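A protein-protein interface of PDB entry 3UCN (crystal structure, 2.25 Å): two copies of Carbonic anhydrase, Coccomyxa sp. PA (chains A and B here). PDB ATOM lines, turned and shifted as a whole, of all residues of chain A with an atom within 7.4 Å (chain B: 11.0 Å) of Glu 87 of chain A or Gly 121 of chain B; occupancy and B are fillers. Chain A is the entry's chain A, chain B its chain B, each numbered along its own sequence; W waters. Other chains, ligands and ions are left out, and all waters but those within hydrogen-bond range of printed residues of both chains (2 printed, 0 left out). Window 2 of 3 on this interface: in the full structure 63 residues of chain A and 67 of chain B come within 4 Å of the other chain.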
ATOM      1  N   LEU A  43      22.007  11.190  15.725  1.00  0.00           N
ATOM      2  CA  LEU A  43      20.690  10.575  15.548  1.00  0.00           C
ATOM      3  C   LEU A  43      20.871   9.409  14.630  1.00  0.00           C
ATOM      4  O   LEU A  43      21.515   9.555  13.637  1.00  0.00           O
ATOM      5  CB  LEU A  43      19.723  11.527  14.870  1.00  0.00           C
ATOM      6  CG  LEU A  43      18.344  11.045  14.380  1.00  0.00           C
ATOM      7  CD1 LEU A  43      17.512  10.301  15.457  1.00  0.00           C
ATOM      8  CD2 LEU A  43      17.544  12.263  13.811  1.00  0.00           C
ATOM      9  N   LEU A  80       4.706  11.904  12.102  1.00  0.00           N
ATOM     10  CA  LEU A  80       5.106  12.705  13.272  1.00  0.00           C
ATOM     11  C   LEU A  80       5.970  11.918  14.271  1.00  0.00           C
ATOM     12  O   LEU A  80       6.645  12.503  15.113  1.00  0.00           O
ATOM     13  CB  LEU A  80       3.875  13.127  13.993  1.00  0.00           C
ATOM     14  CG  LEU A  80       3.084  14.180  13.223  1.00  0.00           C
ATOM     15  CD1 LEU A  80       1.781  14.305  13.924  1.00  0.00           C
ATOM     16  CD2 LEU A  80       3.780  15.525  13.165  1.00  0.00           C
ATOM     17  N   CYS A  82       8.590   9.705  13.367  1.00  0.00           N
ATOM     18  CA  CYS A  82       9.955   9.921  12.913  1.00  0.00           C
ATOM     19  C   CYS A  82      10.315  11.418  12.963  1.00  0.00           C
ATOM     20  O   CYS A  82      11.405  11.763  13.353  1.00  0.00           O
ATOM     21  CB  CYS A  82      10.129   9.462  11.451  1.00  0.00           C
ATOM     22  SG  CYS A  82      11.861   9.574  10.964  1.00  0.00           S
ATOM     23  N   MET A  83       9.401  12.284  12.570  1.00  0.00           N
ATOM     24  CA  MET A  83       9.676  13.731  12.493  1.00  0.00           C
ATOM     25  C   MET A  83       9.979  14.362  13.871  1.00  0.00           C
ATOM     26  O   MET A  83      10.828  15.251  13.950  1.00  0.00           O
ATOM     27  CB  MET A  83       8.515  14.523  11.848  1.00  0.00           C
ATOM     28  CG  MET A  83       8.488  14.429  10.344  1.00  0.00           C
ATOM     29  SD  MET A  83       9.937  15.209   9.485  1.00  0.00           S
ATOM     30  CE  MET A  83      10.954  13.879   9.231  1.00  0.00           C
ATOM     31  N   SER A  84       9.281  13.941  14.939  1.00  0.00           N
ATOM     32  CA  SER A  84       9.627  14.472  16.256  1.00  0.00           C
ATOM     33  C   SER A  84      10.985  13.983  16.801  1.00  0.00           C
ATOM     34  O   SER A  84      11.664  14.731  17.512  1.00  0.00           O
ATOM     35  CB  SER A  84       8.517  14.241  17.271  1.00  0.00           C
ATOM     36  OG  SER A  84       8.333  12.881  17.446  1.00  0.00           O
ATOM     37  N   CYS A  85      11.397  12.769  16.483  1.00  0.00           N
ATOM     38  CA  CYS A  85      12.746  12.366  16.691  1.00  0.00           C
ATOM     39  C   CYS A  85      13.727  13.253  15.992  1.00  0.00           C
ATOM     40  O   CYS A  85      14.771  13.583  16.580  1.00  0.00           O
ATOM     41  CB  CYS A  85      13.015  10.980  16.175  1.00  0.00           C
ATOM     42  SG  CYS A  85      12.342   9.760  17.269  1.00  0.00           S
ATOM     43  N   LEU A  86      13.411  13.664  14.769  1.00  0.00           N
ATOM     44  CA  LEU A  86      14.265  14.516  14.029  1.00  0.00           C
ATOM     45  C   LEU A  86      14.343  15.966  14.607  1.00  0.00           C
ATOM     46  O   LEU A  86      15.454  16.529  14.814  1.00  0.00           O
ATOM     47  CB  LEU A  86      13.824  14.472  12.571  1.00  0.00           C
ATOM     48  CG  LEU A  86      14.640  14.884  11.367  1.00  0.00           C
ATOM     49  CD1 LEU A  86      16.103  14.514  11.459  1.00  0.00           C
ATOM     50  CD2 LEU A  86      14.031  14.117  10.201  1.00  0.00           C
ATOM     51  N   GLU A  87      13.184  16.577  14.808  1.00  0.00           N
ATOM     52  CA  GLU A  87      13.101  17.893  15.394  1.00  0.00           C
ATOM     53  C   GLU A  87      13.710  17.926  16.791  1.00  0.00           C
ATOM     54  O   GLU A  87      14.468  18.855  17.098  1.00  0.00           O
ATOM     55  CB  GLU A  87      11.666  18.347  15.487  1.00  0.00           C
ATOM     56  CG  GLU A  87      11.518  19.800  15.939  1.00  0.00           C
ATOM     57  CD  GLU A  87      10.108  20.126  16.306  1.00  0.00           C
ATOM     58  OE1 GLU A  87       9.684  19.698  17.410  1.00  0.00           O
ATOM     59  OE2 GLU A  87       9.417  20.767  15.474  1.00  0.00           O
ATOM     60  N   TYR A  88      13.382  16.979  17.666  1.00  0.00           N
ATOM     61  CA  TYR A  88      13.899  17.034  19.024  1.00  0.00           C
ATOM     62  C   TYR A  88      15.473  16.984  19.109  1.00  0.00           C
ATOM     63  O   TYR A  88      16.073  17.666  19.938  1.00  0.00           O
ATOM     64  CB  TYR A  88      13.316  15.937  19.880  1.00  0.00           C
ATOM     65  CG  TYR A  88      13.564  16.092  21.380  1.00  0.00           C
ATOM     66  CD1 TYR A  88      12.965  17.154  22.111  1.00  0.00           C
ATOM     67  CD2 TYR A  88      14.357  15.173  22.079  1.00  0.00           C
ATOM     68  CE1 TYR A  88      13.192  17.301  23.497  1.00  0.00           C
ATOM     69  CE2 TYR A  88      14.605  15.308  23.460  1.00  0.00           C
ATOM     70  CZ  TYR A  88      14.009  16.363  24.176  1.00  0.00           C
ATOM     71  OH  TYR A  88      14.207  16.490  25.568  1.00  0.00           O
ATOM     72  N   THR A  89      16.105  16.151  18.300  1.00  0.00           N
ATOM     73  CA  THR A  89      17.540  16.011  18.323  1.00  0.00           C
ATOM     74  C   THR A  89      18.268  17.161  17.620  1.00  0.00           C
ATOM     75  O   THR A  89      19.365  17.519  18.041  1.00  0.00           O
ATOM     76  CB  THR A  89      18.022  14.693  17.687  1.00  0.00           C
ATOM     77  OG1 THR A  89      17.606  14.665  16.318  1.00  0.00           O
ATOM     78  CG2 THR A  89      17.423  13.533  18.429  1.00  0.00           C
ATOM     79  N   VAL A  90      17.703  17.708  16.558  1.00  0.00           N
ATOM     80  CA  VAL A  90      18.364  18.787  15.834  1.00  0.00           C
ATOM     81  C   VAL A  90      18.090  20.163  16.503  1.00  0.00           C
ATOM     82  O   VAL A  90      19.002  20.983  16.662  1.00  0.00           O
ATOM     83  CB  VAL A  90      17.900  18.851  14.379  1.00  0.00           C
ATOM     84  CG1 VAL A  90      18.364  20.173  13.658  1.00  0.00           C
ATOM     85  CG2 VAL A  90      18.269  17.557  13.567  1.00  0.00           C
ATOM     86  N   ASP A  91      16.838  20.442  16.862  1.00  0.00           N
ATOM     87  CA  ASP A  91      16.468  21.709  17.454  1.00  0.00           C
ATOM     88  C   ASP A  91      16.828  21.807  18.969  1.00  0.00           C
ATOM     89  O   ASP A  91      17.286  22.865  19.442  1.00  0.00           O
ATOM     90  CB  ASP A  91      14.996  22.034  17.200  1.00  0.00           C
ATOM     91  CG  ASP A  91      14.724  22.504  15.765  1.00  0.00           C
ATOM     92  OD1 ASP A  91      15.606  22.453  14.875  1.00  0.00           O
ATOM     93  OD2 ASP A  91      13.573  22.883  15.470  1.00  0.00           O
ATOM     94  N   HIS A  92      16.640  20.732  19.733  1.00  0.00           N
ATOM     95  CA  HIS A  92      16.774  20.790  21.193  1.00  0.00           C
ATOM     96  C   HIS A  92      18.102  20.250  21.584  1.00  0.00           C
ATOM     97  O   HIS A  92      18.791  20.910  22.300  1.00  0.00           O
ATOM     98  CB  HIS A  92      15.639  20.087  21.938  1.00  0.00           C
ATOM     99  CG  HIS A  92      14.321  20.762  21.762  1.00  0.00           C
ATOM    100  ND1 HIS A  92      13.806  21.653  22.687  1.00  0.00           N
ATOM    101  CD2 HIS A  92      13.420  20.708  20.749  1.00  0.00           C
ATOM    102  CE1 HIS A  92      12.639  22.106  22.251  1.00  0.00           C
ATOM    103  NE2 HIS A  92      12.395  21.568  21.066  1.00  0.00           N
ATOM    104  N   LEU A  93      18.508  19.087  21.116  1.00  0.00           N
ATOM    105  CA  LEU A  93      19.731  18.529  21.647  1.00  0.00           C
ATOM    106  C   LEU A  93      20.963  18.982  20.865  1.00  0.00           C
ATOM    107  O   LEU A  93      22.105  18.695  21.255  1.00  0.00           O
ATOM    108  CB  LEU A  93      19.667  17.004  21.653  1.00  0.00           C
ATOM    109  CG  LEU A  93      18.584  16.354  22.540  1.00  0.00           C
ATOM    110  CD1 LEU A  93      18.645  14.819  22.485  1.00  0.00           C
ATOM    111  CD2 LEU A  93      18.659  16.840  23.993  1.00  0.00           C
ATOM    112  N   LYS A  94      20.753  19.605  19.715  1.00  0.00           N
ATOM    113  CA  LYS A  94      21.888  19.971  18.792  1.00  0.00           C
ATOM    114  C   LYS A  94      22.846  18.846  18.450  1.00  0.00           C
ATOM    115  O   LYS A  94      24.074  18.992  18.570  1.00  0.00           O
ATOM    116  CB  LYS A  94      22.639  21.250  19.227  1.00  0.00           C
ATOM    117  CG  LYS A  94      21.647  22.415  19.407  1.00  0.00           C
ATOM    118  CD  LYS A  94      22.243  23.716  19.900  1.00  0.00           C
ATOM    119  CE  LYS A  94      21.372  24.352  21.019  1.00  0.00           C
ATOM    120  NZ  LYS A  94      19.876  24.379  20.705  1.00  0.00           N
ATOM    121  N   ILE A 170      13.118  20.279   8.884  1.00  0.00           N
ATOM    122  CA  ILE A 170      13.981  20.375  10.022  1.00  0.00           C
ATOM    123  C   ILE A 170      15.462  20.566   9.613  1.00  0.00           C
ATOM    124  O   ILE A 170      16.168  21.453  10.156  1.00  0.00           O
ATOM    125  CB  ILE A 170      13.853  19.065  10.927  1.00  0.00           C
ATOM    126  CG1 ILE A 170      12.367  18.746  11.341  1.00  0.00           C
ATOM    127  CG2 ILE A 170      14.886  19.053  12.102  1.00  0.00           C
ATOM    128  CD1 ILE A 170      11.590  19.912  11.895  1.00  0.00           C
ATOM    129  N   VAL A 171      15.953  19.683   8.732  1.00  0.00           N
ATOM    130  CA  VAL A 171      17.313  19.745   8.266  1.00  0.00           C
ATOM    131  C   VAL A 171      17.514  20.992   7.373  1.00  0.00           C
ATOM    132  O   VAL A 171      18.533  21.654   7.475  1.00  0.00           O
ATOM    133  CB  VAL A 171      17.666  18.487   7.519  1.00  0.00           C
ATOM    134  CG1 VAL A 171      19.032  18.594   6.823  1.00  0.00           C
ATOM    135  CG2 VAL A 171      17.664  17.338   8.515  1.00  0.00           C
ATOM    136  N   ARG A 177      20.208  28.220   8.869  1.00  0.00           N
ATOM    137  CA  ARG A 177      20.604  29.078   9.980  1.00  0.00           C
ATOM    138  C   ARG A 177      22.057  28.772  10.377  1.00  0.00           C
ATOM    139  O   ARG A 177      22.530  29.194  11.413  1.00  0.00           O
ATOM    140  CB  ARG A 177      19.601  29.027  11.175  1.00  0.00           C
ATOM    141  CG  ARG A 177      19.817  27.833  12.109  1.00  0.00           C
ATOM    142  CD  ARG A 177      18.666  27.601  13.102  1.00  0.00           C
ATOM    143  NE  ARG A 177      18.781  26.261  13.742  1.00  0.00           N
ATOM    144  CZ  ARG A 177      17.810  25.337  13.715  1.00  0.00           C
ATOM    145  NH1 ARG A 177      16.655  25.613  13.111  1.00  0.00           N
ATOM    146  NH2 ARG A 177      17.973  24.159  14.297  1.00  0.00           N
ATOM    147  N   ALA B  48      13.103   6.974  22.446  1.00  0.00           N
ATOM    148  CA  ALA B  48      14.251   7.266  21.592  1.00  0.00           C
ATOM    149  C   ALA B  48      15.529   7.811  22.360  1.00  0.00           C
ATOM    150  O   ALA B  48      16.604   7.860  21.788  1.00  0.00           O
ATOM    151  CB  ALA B  48      13.840   8.275  20.580  1.00  0.00           C
ATOM    152  N   VAL B  71       9.746   9.149  20.745  1.00  0.00           N
ATOM    153  CA  VAL B  71       9.917  10.082  21.829  1.00  0.00           C
ATOM    154  C   VAL B  71       8.786   9.891  22.817  1.00  0.00           C
ATOM    155  O   VAL B  71       7.646  10.217  22.497  1.00  0.00           O
ATOM    156  CB  VAL B  71       9.901  11.547  21.243  1.00  0.00           C
ATOM    157  CG1 VAL B  71       9.716  12.598  22.359  1.00  0.00           C
ATOM    158  CG2 VAL B  71      11.145  11.807  20.386  1.00  0.00           C
ATOM    159  N   ALA B 111       8.304  17.488  29.168  1.00  0.00           N
ATOM    160  CA  ALA B 111       7.661  18.385  28.233  1.00  0.00           C
ATOM    161  C   ALA B 111       6.123  18.266  28.351  1.00  0.00           C
ATOM    162  O   ALA B 111       5.391  19.263  28.265  1.00  0.00           O
ATOM    163  CB  ALA B 111       8.133  18.072  26.833  1.00  0.00           C
ATOM    164  N   TRP B 115       5.243  22.162  29.016  1.00  0.00           N
ATOM    165  CA  TRP B 115       5.034  23.032  27.872  1.00  0.00           C
ATOM    166  C   TRP B 115       3.608  23.525  27.729  1.00  0.00           C
ATOM    167  O   TRP B 115       2.620  22.829  28.048  1.00  0.00           O
ATOM    168  CB  TRP B 115       5.410  22.382  26.581  1.00  0.00           C
ATOM    169  CG  TRP B 115       6.825  22.090  26.402  1.00  0.00           C
ATOM    170  CD1 TRP B 115       7.839  22.292  27.288  1.00  0.00           C
ATOM    171  CD2 TRP B 115       7.394  21.441  25.269  1.00  0.00           C
ATOM    172  NE1 TRP B 115       9.029  21.820  26.756  1.00  0.00           N
ATOM    173  CE2 TRP B 115       8.776  21.312  25.507  1.00  0.00           C
ATOM    174  CE3 TRP B 115       6.876  20.981  24.061  1.00  0.00           C
ATOM    175  CZ2 TRP B 115       9.637  20.724  24.583  1.00  0.00           C
ATOM    176  CZ3 TRP B 115       7.756  20.415  23.119  1.00  0.00           C
ATOM    177  CH2 TRP B 115       9.110  20.292  23.391  1.00  0.00           C
ATOM    178  N   HIS B 116       3.489  24.748  27.228  1.00  0.00           N
ATOM    179  CA  HIS B 116       2.190  25.294  26.910  1.00  0.00           C
ATOM    180  C   HIS B 116       1.870  24.730  25.536  1.00  0.00           C
ATOM    181  O   HIS B 116       2.752  24.650  24.677  1.00  0.00           O
ATOM    182  CB  HIS B 116       2.300  26.830  26.772  1.00  0.00           C
ATOM    183  CG  HIS B 116       0.981  27.529  26.734  1.00  0.00           C
ATOM    184  ND1 HIS B 116       0.254  27.703  25.570  1.00  0.00           N
ATOM    185  CD2 HIS B 116       0.259  28.117  27.719  1.00  0.00           C
ATOM    186  CE1 HIS B 116      -0.864  28.352  25.844  1.00  0.00           C
ATOM    187  NE2 HIS B 116      -0.872  28.638  27.138  1.00  0.00           N
ATOM    188  N   PRO B 117       0.609  24.429  25.301  1.00  0.00           N
ATOM    189  CA  PRO B 117       0.126  23.935  24.028  1.00  0.00           C
ATOM    190  C   PRO B 117       0.409  24.805  22.801  1.00  0.00           C
ATOM    191  O   PRO B 117       0.532  24.287  21.707  1.00  0.00           O
ATOM    192  CB  PRO B 117      -1.407  23.785  24.258  1.00  0.00           C
ATOM    193  CG  PRO B 117      -1.553  23.515  25.679  1.00  0.00           C
ATOM    194  CD  PRO B 117      -0.415  24.341  26.366  1.00  0.00           C
ATOM    195  N   LYS B 118       0.536  26.119  22.963  1.00  0.00           N
ATOM    196  CA  LYS B 118       0.879  26.998  21.806  1.00  0.00           C
ATOM    197  C   LYS B 118       2.278  26.728  21.275  1.00  0.00           C
ATOM    198  O   LYS B 118       2.578  27.152  20.207  1.00  0.00           O
ATOM    199  CB  LYS B 118       0.720  28.487  22.177  1.00  0.00           C
ATOM    200  CG  LYS B 118       1.753  29.108  23.200  1.00  0.00           C
ATOM    201  CD  LYS B 118       1.502  30.659  23.270  1.00  0.00           C
ATOM    202  CE  LYS B 118       2.743  31.449  23.771  1.00  0.00           C
ATOM    203  NZ  LYS B 118       2.807  31.259  25.212  1.00  0.00           N
ATOM    204  N   THR B 119       3.151  26.066  22.013  1.00  0.00           N
ATOM    205  CA  THR B 119       4.530  25.793  21.490  1.00  0.00           C
ATOM    206  C   THR B 119       4.516  25.236  20.026  1.00  0.00           C
ATOM    207  O   THR B 119       3.733  24.313  19.685  1.00  0.00           O
ATOM    208  CB  THR B 119       5.218  24.787  22.355  1.00  0.00           C
ATOM    209  OG1 THR B 119       5.122  25.245  23.687  1.00  0.00           O
ATOM    210  CG2 THR B 119       6.744  24.593  21.997  1.00  0.00           C
ATOM    211  N   ALA B 120       5.358  25.816  19.172  1.00  0.00           N
ATOM    212  CA  ALA B 120       5.342  25.462  17.764  1.00  0.00           C
ATOM    213  C   ALA B 120       6.166  24.182  17.510  1.00  0.00           C
ATOM    214  O   ALA B 120       6.951  23.757  18.364  1.00  0.00           O
ATOM    215  CB  ALA B 120       5.875  26.692  16.875  1.00  0.00           C
ATOM    216  N   GLY B 121       5.971  23.585  16.329  1.00  0.00           N
ATOM    217  CA  GLY B 121       6.785  22.420  15.917  1.00  0.00           C
ATOM    218  C   GLY B 121       6.050  21.074  16.128  1.00  0.00           C
ATOM    219  O   GLY B 121       4.939  20.990  16.727  1.00  0.00           O
ATOM    220  N   VAL B 122       6.697  20.004  15.691  1.00  0.00           N
ATOM    221  CA  VAL B 122       6.060  18.744  15.665  1.00  0.00           C
ATOM    222  C   VAL B 122       6.173  17.970  16.977  1.00  0.00           C
ATOM    223  O   VAL B 122       5.251  17.211  17.249  1.00  0.00           O
ATOM    224  CB  VAL B 122       6.532  17.855  14.445  1.00  0.00           C
ATOM    225  CG1 VAL B 122       6.264  18.624  13.110  1.00  0.00           C
ATOM    226  CG2 VAL B 122       7.947  17.537  14.612  1.00  0.00           C
ATOM    227  N   THR B 123       7.251  18.143  17.759  1.00  0.00           N
ATOM    228  CA  THR B 123       7.395  17.469  19.045  1.00  0.00           C
ATOM    229  C   THR B 123       6.197  17.806  19.924  1.00  0.00           C
ATOM    230  O   THR B 123       5.613  16.925  20.564  1.00  0.00           O
ATOM    231  CB  THR B 123       8.751  17.751  19.748  1.00  0.00           C
ATOM    232  OG1 THR B 123       9.862  17.487  18.858  1.00  0.00           O
ATOM    233  CG2 THR B 123       8.954  16.895  20.996  1.00  0.00           C
ATOM    234  N   ASN B 124       5.780  19.051  19.914  1.00  0.00           N
ATOM    235  CA  ASN B 124       4.643  19.439  20.741  1.00  0.00           C
ATOM    236  C   ASN B 124       3.328  18.752  20.295  1.00  0.00           C
ATOM    237  O   ASN B 124       2.549  18.399  21.128  1.00  0.00           O
ATOM    238  CB  ASN B 124       4.445  20.954  20.721  1.00  0.00           C
ATOM    239  CG  ASN B 124       3.332  21.422  21.652  1.00  0.00           C
ATOM    240  OD1 ASN B 124       3.342  21.120  22.858  1.00  0.00           O
ATOM    241  ND2 ASN B 124       2.392  22.215  21.118  1.00  0.00           N
ATOM    242  N   LEU B 125       3.059  18.635  18.999  1.00  0.00           N
ATOM    243  CA  LEU B 125       1.932  17.834  18.502  1.00  0.00           C
ATOM    244  C   LEU B 125       2.035  16.375  18.983  1.00  0.00           C
ATOM    245  O   LEU B 125       1.117  15.853  19.616  1.00  0.00           O
ATOM    246  CB  LEU B 125       1.941  17.848  16.993  1.00  0.00           C
ATOM    247  CG  LEU B 125       1.744  19.241  16.417  1.00  0.00           C
ATOM    248  CD1 LEU B 125       1.808  19.096  14.932  1.00  0.00           C
ATOM    249  CD2 LEU B 125       0.337  19.866  16.866  1.00  0.00           C
ATOM    250  N   TRP B 126       3.197  15.777  18.733  1.00  0.00           N
ATOM    251  CA  TRP B 126       3.478  14.428  19.063  1.00  0.00           C
ATOM    252  C   TRP B 126       3.239  14.063  20.530  1.00  0.00           C
ATOM    253  O   TRP B 126       2.660  12.994  20.854  1.00  0.00           O
ATOM    254  CB  TRP B 126       4.915  14.063  18.622  1.00  0.00           C
ATOM    255  CG  TRP B 126       5.275  12.681  19.039  1.00  0.00           C
ATOM    256  CD1 TRP B 126       6.065  12.337  20.050  1.00  0.00           C
ATOM    257  CD2 TRP B 126       4.825  11.440  18.419  1.00  0.00           C
ATOM    258  NE1 TRP B 126       6.145  10.938  20.147  1.00  0.00           N
ATOM    259  CE2 TRP B 126       5.389  10.373  19.162  1.00  0.00           C
ATOM    260  CE3 TRP B 126       3.981  11.141  17.323  1.00  0.00           C
ATOM    261  CZ2 TRP B 126       5.188   9.011  18.832  1.00  0.00           C
ATOM    262  CZ3 TRP B 126       3.746   9.773  16.998  1.00  0.00           C
ATOM    263  CH2 TRP B 126       4.365   8.732  17.765  1.00  0.00           C
ATOM    264  N   ILE B 127       3.683  14.918  21.450  1.00  0.00           N
ATOM    265  CA  ILE B 127       3.535  14.554  22.874  1.00  0.00           C
ATOM    266  C   ILE B 127       2.102  14.849  23.389  1.00  0.00           C
ATOM    267  O   ILE B 127       1.865  14.741  24.573  1.00  0.00           O
ATOM    268  CB  ILE B 127       4.590  15.279  23.805  1.00  0.00           C
ATOM    269  CG1 ILE B 127       4.374  16.786  23.671  1.00  0.00           C
ATOM    270  CG2 ILE B 127       6.032  14.869  23.415  1.00  0.00           C
ATOM    271  CD1 ILE B 127       4.754  17.548  24.795  1.00  0.00           C
ATOM    272  N   SER B 128       1.158  15.211  22.518  1.00  0.00           N
ATOM    273  CA  SER B 128      -0.192  15.322  22.990  1.00  0.00           C
ATOM    274  C   SER B 128      -0.645  14.104  23.765  1.00  0.00           C
ATOM    275  O   SER B 128      -1.377  14.286  24.686  1.00  0.00           O
ATOM    276  CB  SER B 128      -1.223  15.616  21.850  1.00  0.00           C
ATOM    277  OG  SER B 128      -0.833  16.722  21.079  1.00  0.00           O
ATOM    278  N   ARG B 131       0.037  14.655  27.403  1.00  0.00           N
ATOM    279  CA  ARG B 131      -0.896  15.524  28.083  1.00  0.00           C
ATOM    280  C   ARG B 131      -2.205  14.837  28.440  1.00  0.00           C
ATOM    281  O   ARG B 131      -2.807  15.157  29.422  1.00  0.00           O
ATOM    282  CB  ARG B 131      -1.145  16.809  27.319  1.00  0.00           C
ATOM    283  CG  ARG B 131      -0.009  17.750  27.339  1.00  0.00           C
ATOM    284  CD  ARG B 131      -0.380  19.064  26.746  1.00  0.00           C
ATOM    285  NE  ARG B 131      -0.432  19.050  25.301  1.00  0.00           N
ATOM    286  CZ  ARG B 131       0.564  19.387  24.512  1.00  0.00           C
ATOM    287  NH1 ARG B 131       1.705  19.760  25.008  1.00  0.00           N
ATOM    288  NH2 ARG B 131       0.419  19.347  23.225  1.00  0.00           N
HETATM  289  O   HOH W   1       8.956  10.070  18.079  1.00  0.00           O
HETATM  290  O   HOH W   2       7.770  21.342  19.115  1.00  0.00           O
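The backbone NH (N) of Val 122 of chain B lies within hydrogen-bond range of the side-chain carboxylate (OE2) of Glu 87 of chain A, 2.8 Å away. OG1 of Thr 123 of chain B is in hydrogen-bond range of OE1 of Glu 87 of chain A (2.6 Å).
O of Leu 80 of chain A sits at hydrogen-bond distance from OG of Ser 84 of chain A, 2.9 Å away. The side-chain hydroxyl of Thr 89 of chain A sits at hydrogen-bond distance from the backbone carbonyl oxygen of Cys 85 of chain A (3.0 Å). The backbone carbonyl oxygen (O) of Tyr 88 of chain A lies within hydrogen-bond range of the backbone NH (N) of Leu 93 of chain A (3.1 Å). The backbone carbonyl oxygen of Val 71 of chain B lies within hydrogen-bond range of the indole nitrogen of Trp 126 of chain B, 2.9 Å away.
Among the printed residues, pairs that only touch across the chains: Glu 87 of chain A with Gly 121 of chain B (3.1 Å), Ser 84 of chain A with Trp 126 of chain B (3.5 Å), Ser 84 of chain A with Thr 123 of chain B (3.6 Å), Leu 80 of chain A with Trp 126 of chain B (3.7 Å), Met 83 of chain A with Val 122 of chain B (3.7 Å), Tyr 88 of chain A with Thr 123 of chain B (3.8 Å), Leu 80 of chain A with Val 122 of chain B (3.8 Å), Ser 84 of chain A with Val 122 of chain B (3.8 Å), Cys 85 of chain A with Val 71 of chain B (3.9 Å) and Cys 85 of chain A with Ala 48 of chain B (3.9 Å).
Glu 87 of chain A touches just these residues of chain B: Gly 121 (3.1 Å), Val 122 (2.8 Å) and Thr 123 (2.6 Å). Met 83 of chain A touches just one residue of chain B: Val 122 (3.7 Å). Ser 84 of chain A touches just these residues of chain B: Val 122, Thr 123 and Trp 126. No residue of chain B comes within 4 Å of Leu 86 of chain A. No residue of chain B comes within 4 Å of Thr 89 of chain A. No residue of chain B comes within 4 Å of Val 90 of chain A. No residue of chain B comes within 4 Å of Asp 91 of chain A. Printed residues of chain A within 4 Å of Ala 48 of chain B: Cys 85 (3.9 Å). Of the printed residues of chain A, Trp 126 of chain B touches Leu 80 and Ser 84. Of the printed residues of chain A, Val 71 of chain B touches Cys 85 (3.9 Å). Of the printed residues of chain A, Thr 123 of chain B touches Ser 84, Glu 87 and Tyr 88. Of the printed residues of chain B, Cys 85 of chain A touches Ala 48 and Val 71. Thr 119 of chain B touches none of the printed residues of chain A. The nearest residue of chain B that does not touch Glu 87 of chain A is Asn 124 of chain B (4.7 Å).
Of the 18 printed residues of chain A, 6 touch a printed residue of chain B. Printed residues of chain A that touch a printed residue of chain B: Leu 80, Met 83, Ser 84, Cys 85, Glu 87 and Tyr 88. Hydrophobic or aromatic side chains of chain A within 4 Å of the printed part of chain B: Leu 80 and Tyr 88. Hydrophobic or aromatic side chains of chain B within 4 Å of the printed part of chain A: Ala 48, Val 71, Val 122 and Trp 126. Among the printed residues, 12 pairs touch across the chains. Among the printed residues, no Asp or Glu carboxylate lies within 4 Å of a Lys or Arg side-chain nitrogen of the other chain.
No position is printed for both chains.
Water W2 lies within hydrogen-bond range of O of Ala 120 of chain B (2.7 Å), OE1 of Glu 87 of chain A (3.0 Å) and N of Asn 124 of chain B (3.1 Å). Water W1 lies within hydrogen-bond range of N of Val 71 of chain B (2.9 Å), OG of Ser 84 of chain A (2.9 Å) and SG of Cys 85 of chain A (3.5 Å).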
